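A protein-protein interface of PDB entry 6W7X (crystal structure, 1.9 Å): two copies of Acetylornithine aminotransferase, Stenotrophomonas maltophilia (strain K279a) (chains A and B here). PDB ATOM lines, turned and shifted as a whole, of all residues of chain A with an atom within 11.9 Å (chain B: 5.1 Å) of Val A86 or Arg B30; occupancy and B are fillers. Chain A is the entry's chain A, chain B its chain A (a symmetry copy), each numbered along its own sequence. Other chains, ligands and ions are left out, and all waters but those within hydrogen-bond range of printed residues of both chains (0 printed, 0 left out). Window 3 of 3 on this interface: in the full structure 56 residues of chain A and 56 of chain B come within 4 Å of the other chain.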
ATOM      1  N   LEU A  80     -19.067  -5.313  15.478  1.00  0.00           N
ATOM      2  CA  LEU A  80     -18.584  -4.423  16.520  1.00  0.00           C
ATOM      3  C   LEU A  80     -17.065  -4.440  16.540  1.00  0.00           C
ATOM      4  O   LEU A  80     -16.455  -5.511  16.630  1.00  0.00           O
ATOM      5  CB  LEU A  80     -19.142  -4.859  17.873  1.00  0.00           C
ATOM      6  CG  LEU A  80     -18.939  -3.912  19.050  1.00  0.00           C
ATOM      7  CD1 LEU A  80     -19.862  -2.715  18.896  1.00  0.00           C
ATOM      8  CD2 LEU A  80     -19.185  -4.658  20.374  1.00  0.00           C
ATOM      9  N   HIS A  82     -15.001  -2.187  18.611  1.00  0.00           N
ATOM     10  CA  HIS A  82     -14.317  -1.512  19.703  1.00  0.00           C
ATOM     11  C   HIS A  82     -15.337  -1.153  20.772  1.00  0.00           C
ATOM     12  O   HIS A  82     -16.450  -0.725  20.454  1.00  0.00           O
ATOM     13  CB  HIS A  82     -13.604  -0.257  19.179  1.00  0.00           C
ATOM     14  CG  HIS A  82     -13.161   0.685  20.251  1.00  0.00           C
ATOM     15  ND1 HIS A  82     -11.995   0.506  20.965  1.00  0.00           N
ATOM     16  CD2 HIS A  82     -13.726   1.822  20.725  1.00  0.00           C
ATOM     17  CE1 HIS A  82     -11.863   1.487  21.839  1.00  0.00           C
ATOM     18  NE2 HIS A  82     -12.896   2.305  21.708  1.00  0.00           N
ATOM     19  N   THR A  83     -14.956  -1.340  22.036  1.00  0.00           N
ATOM     20  CA  THR A  83     -15.802  -0.998  23.167  1.00  0.00           C
ATOM     21  C   THR A  83     -15.184   0.015  24.111  1.00  0.00           C
ATOM     22  O   THR A  83     -15.930   0.741  24.782  1.00  0.00           O
ATOM     23  CB  THR A  83     -16.122  -2.245  23.993  1.00  0.00           C
ATOM     24  OG1 THR A  83     -14.894  -2.765  24.515  1.00  0.00           O
ATOM     25  CG2 THR A  83     -16.792  -3.294  23.131  1.00  0.00           C
ATOM     26  N   SER A  84     -13.849   0.077  24.169  1.00  0.00           N
ATOM     27  CA  SER A  84     -13.061   0.709  25.225  1.00  0.00           C
ATOM     28  C   SER A  84     -13.079  -0.190  26.444  1.00  0.00           C
ATOM     29  O   SER A  84     -13.828  -1.173  26.483  1.00  0.00           O
ATOM     30  CB  SER A  84     -13.571   2.107  25.601  1.00  0.00           C
ATOM     31  OG  SER A  84     -14.696   2.020  26.472  1.00  0.00           O
ATOM     32  N   ASN A  85     -12.258   0.127  27.440  1.00  0.00           N
ATOM     33  CA  ASN A  85     -12.244  -0.682  28.655  1.00  0.00           C
ATOM     34  C   ASN A  85     -13.401  -0.353  29.586  1.00  0.00           C
ATOM     35  O   ASN A  85     -13.526  -0.976  30.645  1.00  0.00           O
ATOM     36  CB  ASN A  85     -10.910  -0.515  29.390  1.00  0.00           C
ATOM     37  CG  ASN A  85     -10.518   0.938  29.583  1.00  0.00           C
ATOM     38  OD1 ASN A  85     -11.348   1.788  29.921  1.00  0.00           O
ATOM     39  ND2 ASN A  85      -9.241   1.232  29.361  1.00  0.00           N
ATOM     40  N   VAL A  86     -14.245   0.610  29.223  1.00  0.00           N
ATOM     41  CA  VAL A  86     -15.388   0.936  30.066  1.00  0.00           C
ATOM     42  C   VAL A  86     -16.490  -0.113  29.925  1.00  0.00           C
ATOM     43  O   VAL A  86     -17.273  -0.328  30.859  1.00  0.00           O
ATOM     44  CB  VAL A  86     -15.878   2.359  29.726  1.00  0.00           C
ATOM     45  CG1 VAL A  86     -17.321   2.582  30.144  1.00  0.00           C
ATOM     46  CG2 VAL A  86     -14.981   3.377  30.404  1.00  0.00           C
ATOM     47  N   PHE A  87     -16.565  -0.785  28.779  1.00  0.00           N
ATOM     48  CA  PHE A  87     -17.587  -1.790  28.516  1.00  0.00           C
ATOM     49  C   PHE A  87     -16.928  -3.103  28.118  1.00  0.00           C
ATOM     50  O   PHE A  87     -15.756  -3.142  27.736  1.00  0.00           O
ATOM     51  CB  PHE A  87     -18.546  -1.354  27.389  1.00  0.00           C
ATOM     52  CG  PHE A  87     -19.065   0.055  27.522  1.00  0.00           C
ATOM     53  CD1 PHE A  87     -20.022   0.370  28.473  1.00  0.00           C
ATOM     54  CD2 PHE A  87     -18.625   1.053  26.663  1.00  0.00           C
ATOM     55  CE1 PHE A  87     -20.511   1.659  28.592  1.00  0.00           C
ATOM     56  CE2 PHE A  87     -19.112   2.350  26.768  1.00  0.00           C
ATOM     57  CZ  PHE A  87     -20.061   2.657  27.732  1.00  0.00           C
ATOM     58  N   TYR A  88     -17.707  -4.177  28.192  1.00  0.00           N
ATOM     59  CA  TYR A  88     -17.265  -5.514  27.829  1.00  0.00           C
ATOM     60  C   TYR A  88     -17.769  -5.909  26.444  1.00  0.00           C
ATOM     61  O   TYR A  88     -18.771  -5.394  25.950  1.00  0.00           O
ATOM     62  CB  TYR A  88     -17.768  -6.543  28.843  1.00  0.00           C
ATOM     63  CG  TYR A  88     -17.092  -6.552  30.195  1.00  0.00           C
ATOM     64  CD1 TYR A  88     -17.747  -6.073  31.323  1.00  0.00           C
ATOM     65  CD2 TYR A  88     -15.822  -7.088  30.354  1.00  0.00           C
ATOM     66  CE1 TYR A  88     -17.146  -6.105  32.569  1.00  0.00           C
ATOM     67  CE2 TYR A  88     -15.211  -7.121  31.595  1.00  0.00           C
ATOM     68  CZ  TYR A  88     -15.875  -6.629  32.698  1.00  0.00           C
ATOM     69  OH  TYR A  88     -15.263  -6.667  33.932  1.00  0.00           O
ATOM     70  N   SER A  89     -17.052  -6.847  25.824  1.00  0.00           N
ATOM     71  CA  SER A  89     -17.561  -7.624  24.700  1.00  0.00           C
ATOM     72  C   SER A  89     -17.069  -9.059  24.868  1.00  0.00           C
ATOM     73  O   SER A  89     -16.168  -9.333  25.664  1.00  0.00           O
ATOM     74  CB  SER A  89     -17.142  -7.048  23.343  1.00  0.00           C
ATOM     75  OG  SER A  89     -15.735  -7.062  23.180  1.00  0.00           O
ATOM     76  N   ALA A  90     -17.663  -9.977  24.103  1.00  0.00           N
ATOM     77  CA  ALA A  90     -17.442 -11.404  24.316  1.00  0.00           C
ATOM     78  C   ALA A  90     -16.116 -11.939  23.767  1.00  0.00           C
ATOM     79  O   ALA A  90     -15.443 -12.697  24.477  1.00  0.00           O
ATOM     80  CB  ALA A  90     -18.620 -12.201  23.738  1.00  0.00           C
ATOM     81  N   PRO A  92     -13.034 -10.763  23.458  1.00  0.00           N
ATOM     82  CA  PRO A  92     -11.892 -10.620  24.386  1.00  0.00           C
ATOM     83  C   PRO A  92     -12.004 -11.502  25.624  1.00  0.00           C
ATOM     84  O   PRO A  92     -10.998 -12.069  26.066  1.00  0.00           O
ATOM     85  CB  PRO A  92     -11.915  -9.121  24.741  1.00  0.00           C
ATOM     86  CG  PRO A  92     -12.698  -8.484  23.649  1.00  0.00           C
ATOM     87  CD  PRO A  92     -13.739  -9.476  23.296  1.00  0.00           C
ATOM     88  N   LEU A  93     -13.204 -11.636  26.197  1.00  0.00           N
ATOM     89  CA  LEU A  93     -13.357 -12.466  27.386  1.00  0.00           C
ATOM     90  C   LEU A  93     -13.046 -13.925  27.077  1.00  0.00           C
ATOM     91  O   LEU A  93     -12.376 -14.602  27.864  1.00  0.00           O
ATOM     92  CB  LEU A  93     -14.768 -12.319  27.955  1.00  0.00           C
ATOM     93  CG  LEU A  93     -15.107 -10.926  28.499  1.00  0.00           C
ATOM     94  CD1 LEU A  93     -16.583 -10.805  28.863  1.00  0.00           C
ATOM     95  CD2 LEU A  93     -14.224 -10.599  29.699  1.00  0.00           C
ATOM     96  N   LEU A 111      -4.605  -7.821  27.549  1.00  0.00           N
ATOM     97  CA  LEU A 111      -4.661  -7.720  26.094  1.00  0.00           C
ATOM     98  C   LEU A 111      -4.325  -6.301  25.657  1.00  0.00           C
ATOM     99  O   LEU A 111      -4.856  -5.329  26.207  1.00  0.00           O
ATOM    100  CB  LEU A 111      -6.042  -8.111  25.565  1.00  0.00           C
ATOM    101  CG  LEU A 111      -6.517  -9.547  25.803  1.00  0.00           C
ATOM    102  CD1 LEU A 111      -7.940  -9.710  25.266  1.00  0.00           C
ATOM    103  CD2 LEU A 111      -5.569 -10.537  25.140  1.00  0.00           C
ATOM    104  N   GLY A 295      -7.302  -5.737  28.653  1.00  0.00           N
ATOM    105  CA  GLY A 295      -8.323  -4.918  28.013  1.00  0.00           C
ATOM    106  C   GLY A 295      -8.825  -5.491  26.694  1.00  0.00           C
ATOM    107  O   GLY A 295      -9.721  -6.338  26.686  1.00  0.00           O
ATOM    108  N   GLY A 296      -8.262  -5.010  25.577  1.00  0.00           N
ATOM    109  CA  GLY A 296      -8.509  -5.600  24.274  1.00  0.00           C
ATOM    110  C   GLY A 296      -9.729  -5.041  23.569  1.00  0.00           C
ATOM    111  O   GLY A 296     -10.473  -4.203  24.085  1.00  0.00           O
ATOM    112  N   ASN A 297      -9.931  -5.524  22.346  1.00  0.00           N
ATOM    113  CA  ASN A 297     -11.056  -5.118  21.511  1.00  0.00           C
ATOM    114  C   ASN A 297     -11.604  -6.345  20.799  1.00  0.00           C
ATOM    115  O   ASN A 297     -10.871  -7.324  20.593  1.00  0.00           O
ATOM    116  CB  ASN A 297     -10.656  -4.030  20.487  1.00  0.00           C
ATOM    117  CG  ASN A 297      -9.689  -4.536  19.418  1.00  0.00           C
ATOM    118  OD1 ASN A 297     -10.107  -5.071  18.387  1.00  0.00           O
ATOM    119  ND2 ASN A 297      -8.400  -4.347  19.650  1.00  0.00           N
ATOM    120  N   PRO A 298     -12.891  -6.340  20.436  1.00  0.00           N
ATOM    121  CA  PRO A 298     -13.484  -7.567  19.869  1.00  0.00           C
ATOM    122  C   PRO A 298     -12.969  -7.916  18.479  1.00  0.00           C
ATOM    123  O   PRO A 298     -13.028  -9.092  18.097  1.00  0.00           O
ATOM    124  CB  PRO A 298     -14.986  -7.257  19.851  1.00  0.00           C
ATOM    125  CG  PRO A 298     -15.071  -5.749  19.810  1.00  0.00           C
ATOM    126  CD  PRO A 298     -13.880  -5.254  20.584  1.00  0.00           C
ATOM    127  N   PRO B  29     -15.118  -1.639  34.937  1.00  0.00           N
ATOM    128  CA  PRO B  29     -15.914  -1.706  33.706  1.00  0.00           C
ATOM    129  C   PRO B  29     -17.387  -1.982  33.989  1.00  0.00           C
ATOM    130  O   PRO B  29     -17.695  -2.807  34.852  1.00  0.00           O
ATOM    131  CB  PRO B  29     -15.282  -2.874  32.934  1.00  0.00           C
ATOM    132  CG  PRO B  29     -13.926  -3.072  33.556  1.00  0.00           C
ATOM    133  CD  PRO B  29     -14.094  -2.696  34.992  1.00  0.00           C
ATOM    134  N   ARG B  30     -18.278  -1.295  33.274  1.00  0.00           N
ATOM    135  CA  ARG B  30     -19.709  -1.534  33.419  1.00  0.00           C
ATOM    136  C   ARG B  30     -20.048  -2.969  33.032  1.00  0.00           C
ATOM    137  O   ARG B  30     -19.591  -3.472  32.002  1.00  0.00           O
ATOM    138  CB  ARG B  30     -20.497  -0.542  32.559  1.00  0.00           C
ATOM    139  CG  ARG B  30     -21.829  -1.074  32.034  1.00  0.00           C
ATOM    140  CD  ARG B  30     -23.029  -0.237  32.489  1.00  0.00           C
ATOM    141  NE  ARG B  30     -22.683   1.163  32.731  1.00  0.00           N
ATOM    142  CZ  ARG B  30     -22.744   1.750  33.922  1.00  0.00           C
ATOM    143  NH1 ARG B  30     -22.407   3.025  34.052  1.00  0.00           N
ATOM    144  NH2 ARG B  30     -23.153   1.063  34.983  1.00  0.00           N
ATOM    145  N   GLN B  31     -20.854  -3.630  33.868  1.00  0.00           N
ATOM    146  CA  GLN B  31     -21.215  -5.034  33.668  1.00  0.00           C
ATOM    147  C   GLN B  31     -22.258  -5.150  32.552  1.00  0.00           C
ATOM    148  O   GLN B  31     -23.412  -5.531  32.761  1.00  0.00           O
ATOM    149  CB  GLN B  31     -21.721  -5.643  34.968  1.00  0.00           C
ATOM    150  N   VAL B  32     -21.822  -4.818  31.336  1.00  0.00           N
ATOM    151  CA  VAL B  32     -22.659  -4.887  30.141  1.00  0.00           C
ATOM    152  C   VAL B  32     -21.805  -5.413  28.994  1.00  0.00           C
ATOM    153  O   VAL B  32     -20.799  -4.794  28.633  1.00  0.00           O
ATOM    154  CB  VAL B  32     -23.271  -3.521  29.774  1.00  0.00           C
ATOM    155  CG1 VAL B  32     -23.704  -3.495  28.315  1.00  0.00           C
ATOM    156  CG2 VAL B  32     -24.453  -3.214  30.682  1.00  0.00           C
ATOM    157  N   ILE B  57     -15.407   5.856  23.972  1.00  0.00           N
ATOM    158  CA  ILE B  57     -14.627   6.999  24.448  1.00  0.00           C
ATOM    159  C   ILE B  57     -14.024   7.755  23.265  1.00  0.00           C
ATOM    160  O   ILE B  57     -12.798   7.813  23.098  1.00  0.00           O
ATOM    161  CB  ILE B  57     -13.551   6.607  25.466  1.00  0.00           C
ATOM    162  CG1 ILE B  57     -14.107   5.583  26.470  1.00  0.00           C
ATOM    163  CG2 ILE B  57     -13.072   7.866  26.196  1.00  0.00           C
ATOM    164  CD1 ILE B  57     -13.136   5.192  27.532  1.00  0.00           C
ATOM    165  N   LEU B 367     -24.618   7.883  35.762  1.00  0.00           N
ATOM    166  CA  LEU B 367     -24.267   6.946  34.696  1.00  0.00           C
ATOM    167  C   LEU B 367     -24.938   5.594  34.906  1.00  0.00           C
ATOM    168  O   LEU B 367     -25.441   4.985  33.954  1.00  0.00           O
ATOM    169  CB  LEU B 367     -22.752   6.765  34.618  1.00  0.00           C
ATOM    170  CG  LEU B 367     -21.911   7.903  34.064  1.00  0.00           C
ATOM    171  CD1 LEU B 367     -20.544   7.361  33.664  1.00  0.00           C
ATOM    172  CD2 LEU B 367     -22.603   8.546  32.894  1.00  0.00           C
ATOM    173  N   ASP B 368     -24.964   5.115  36.151  1.00  0.00           N
ATOM    174  CA  ASP B 368     -25.682   3.882  36.447  1.00  0.00           C
ATOM    175  C   ASP B 368     -27.163   3.999  36.094  1.00  0.00           C
ATOM    176  O   ASP B 368     -27.745   3.078  35.511  1.00  0.00           O
ATOM    177  CB  ASP B 368     -25.492   3.514  37.918  1.00  0.00           C
ATOM    178  CG  ASP B 368     -24.093   2.992  38.213  1.00  0.00           C
ATOM    179  OD1 ASP B 368     -23.450   2.457  37.286  1.00  0.00           O
ATOM    180  OD2 ASP B 368     -23.638   3.114  39.368  1.00  0.00           O
ATOM    181  N   ALA B 371     -27.518   3.784  32.215  1.00  0.00           N
ATOM    182  CA  ALA B 371     -27.510   2.426  31.679  1.00  0.00           C
ATOM    183  C   ALA B 371     -28.851   1.750  31.906  1.00  0.00           C
ATOM    184  O   ALA B 371     -29.369   1.060  31.018  1.00  0.00           O
ATOM    185  CB  ALA B 371     -26.379   1.604  32.306  1.00  0.00           C
ATOM    186  N   LEU B 376     -25.790   4.669  27.079  1.00  0.00           N
ATOM    187  CA  LEU B 376     -24.379   4.560  27.424  1.00  0.00           C
ATOM    188  C   LEU B 376     -23.736   5.929  27.264  1.00  0.00           C
ATOM    189  O   LEU B 376     -23.736   6.505  26.171  1.00  0.00           O
ATOM    190  CB  LEU B 376     -23.657   3.539  26.547  1.00  0.00           C
ATOM    191  CG  LEU B 376     -24.231   2.132  26.556  1.00  0.00           C
ATOM    192  CD1 LEU B 376     -23.396   1.235  25.656  1.00  0.00           C
ATOM    193  CD2 LEU B 376     -24.275   1.587  27.979  1.00  0.00           C
ATOM    194  N   LEU B 378     -20.578   8.692  29.428  1.00  0.00           N
ATOM    195  CA  LEU B 378     -19.350   8.678  30.199  1.00  0.00           C
ATOM    196  C   LEU B 378     -19.370   9.761  31.265  1.00  0.00           C
ATOM    197  O   LEU B 378     -20.216  10.656  31.271  1.00  0.00           O
ATOM    198  CB  LEU B 378     -18.127   8.893  29.300  1.00  0.00           C
ATOM    199  CG  LEU B 378     -17.927   7.900  28.164  1.00  0.00           C
ATOM    200  CD1 LEU B 378     -16.821   8.415  27.269  1.00  0.00           C
ATOM    201  CD2 LEU B 378     -17.596   6.505  28.712  1.00  0.00           C
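The backbone NH of Arg B30 sits at hydrogen-bond distance from the backbone carbonyl oxygen of Val A86. O of Val B32 is in hydrogen-bond range of N of Tyr A88 (3.2 Å).
N of Ser A84 lies close to NE2 of His A82 (3.5 Å). OG1 of Thr A83 is in hydrogen-bond range of O of Phe A87 (3.4 Å). OG of Ser A84 lies close to N of Val A86 (3.1 Å). OD1 of Asp B368 lies within salt-bridge range of NH2 of Arg B30 (2.7 Å).
Among the printed residues, pairs that only touch across the chains: Tyr A88 with Arg B30, Val A86 with Pro B29, Asn A85 with Pro B29, Ser A84 with Ile B57, Tyr A88 with Pro B29, Phe A87 with Leu B376 and Val A86 with Ile B57.
Of chain B, only Pro B29 (3.4 Å), Arg B30 (2.8 Å) and Ile B57 (3.9 Å) come within 4 Å of Val A86. Of the printed residues of chain A, Pro B29 touches Asn A85 (3.5 Å), Val A86 (3.4 Å) and Tyr A88 (3.7 Å). No residue of chain A comes within 4 Å of Gln B31. Of chain A, only Tyr A88 comes within 4 Å of Val B32. Leu B367 touches none of the printed residues of chain A. Ala B371 touches none of the printed residues of chain A. Printed residues of chain B within 4 Å of Phe A87: Leu B376. Of the printed residues of chain B, Tyr A88 touches Pro B29 (3.7 Å), Arg B30 (3.3 Å) and Val B32 (3.2 Å). Printed residues of chain B within 4 Å of Ser A84: Ile B57 (3.6 Å). Of the printed residues of chain A, Ile B57 touches Ser A84 and Val A86. Gly A296 touches none of the printed residues of chain B. Pro A298 touches none of the printed residues of chain B. The nearest residue of chain B that does not touch Val A86 is Leu B378 (4.2 Å).
Of the 10 printed residues of chain B, 5 touch a printed residue of chain A. Hydrophobic or aromatic side chains of chain B within 4 Å of the printed part of chain A: Pro B29, Ile B57 and Leu B376. Printed residues of chain A that touch a printed residue of chain B: Ser A84, Asn A85, Val A86, Phe A87 and Tyr A88. Along chain A the printed residues that touch a printed residue of chain B span positions 84 to 88.
No position is printed for both chains. Of the 9 pairs that touch across the chains among the printed residues, none has its exchanged pair printed and touching as well.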
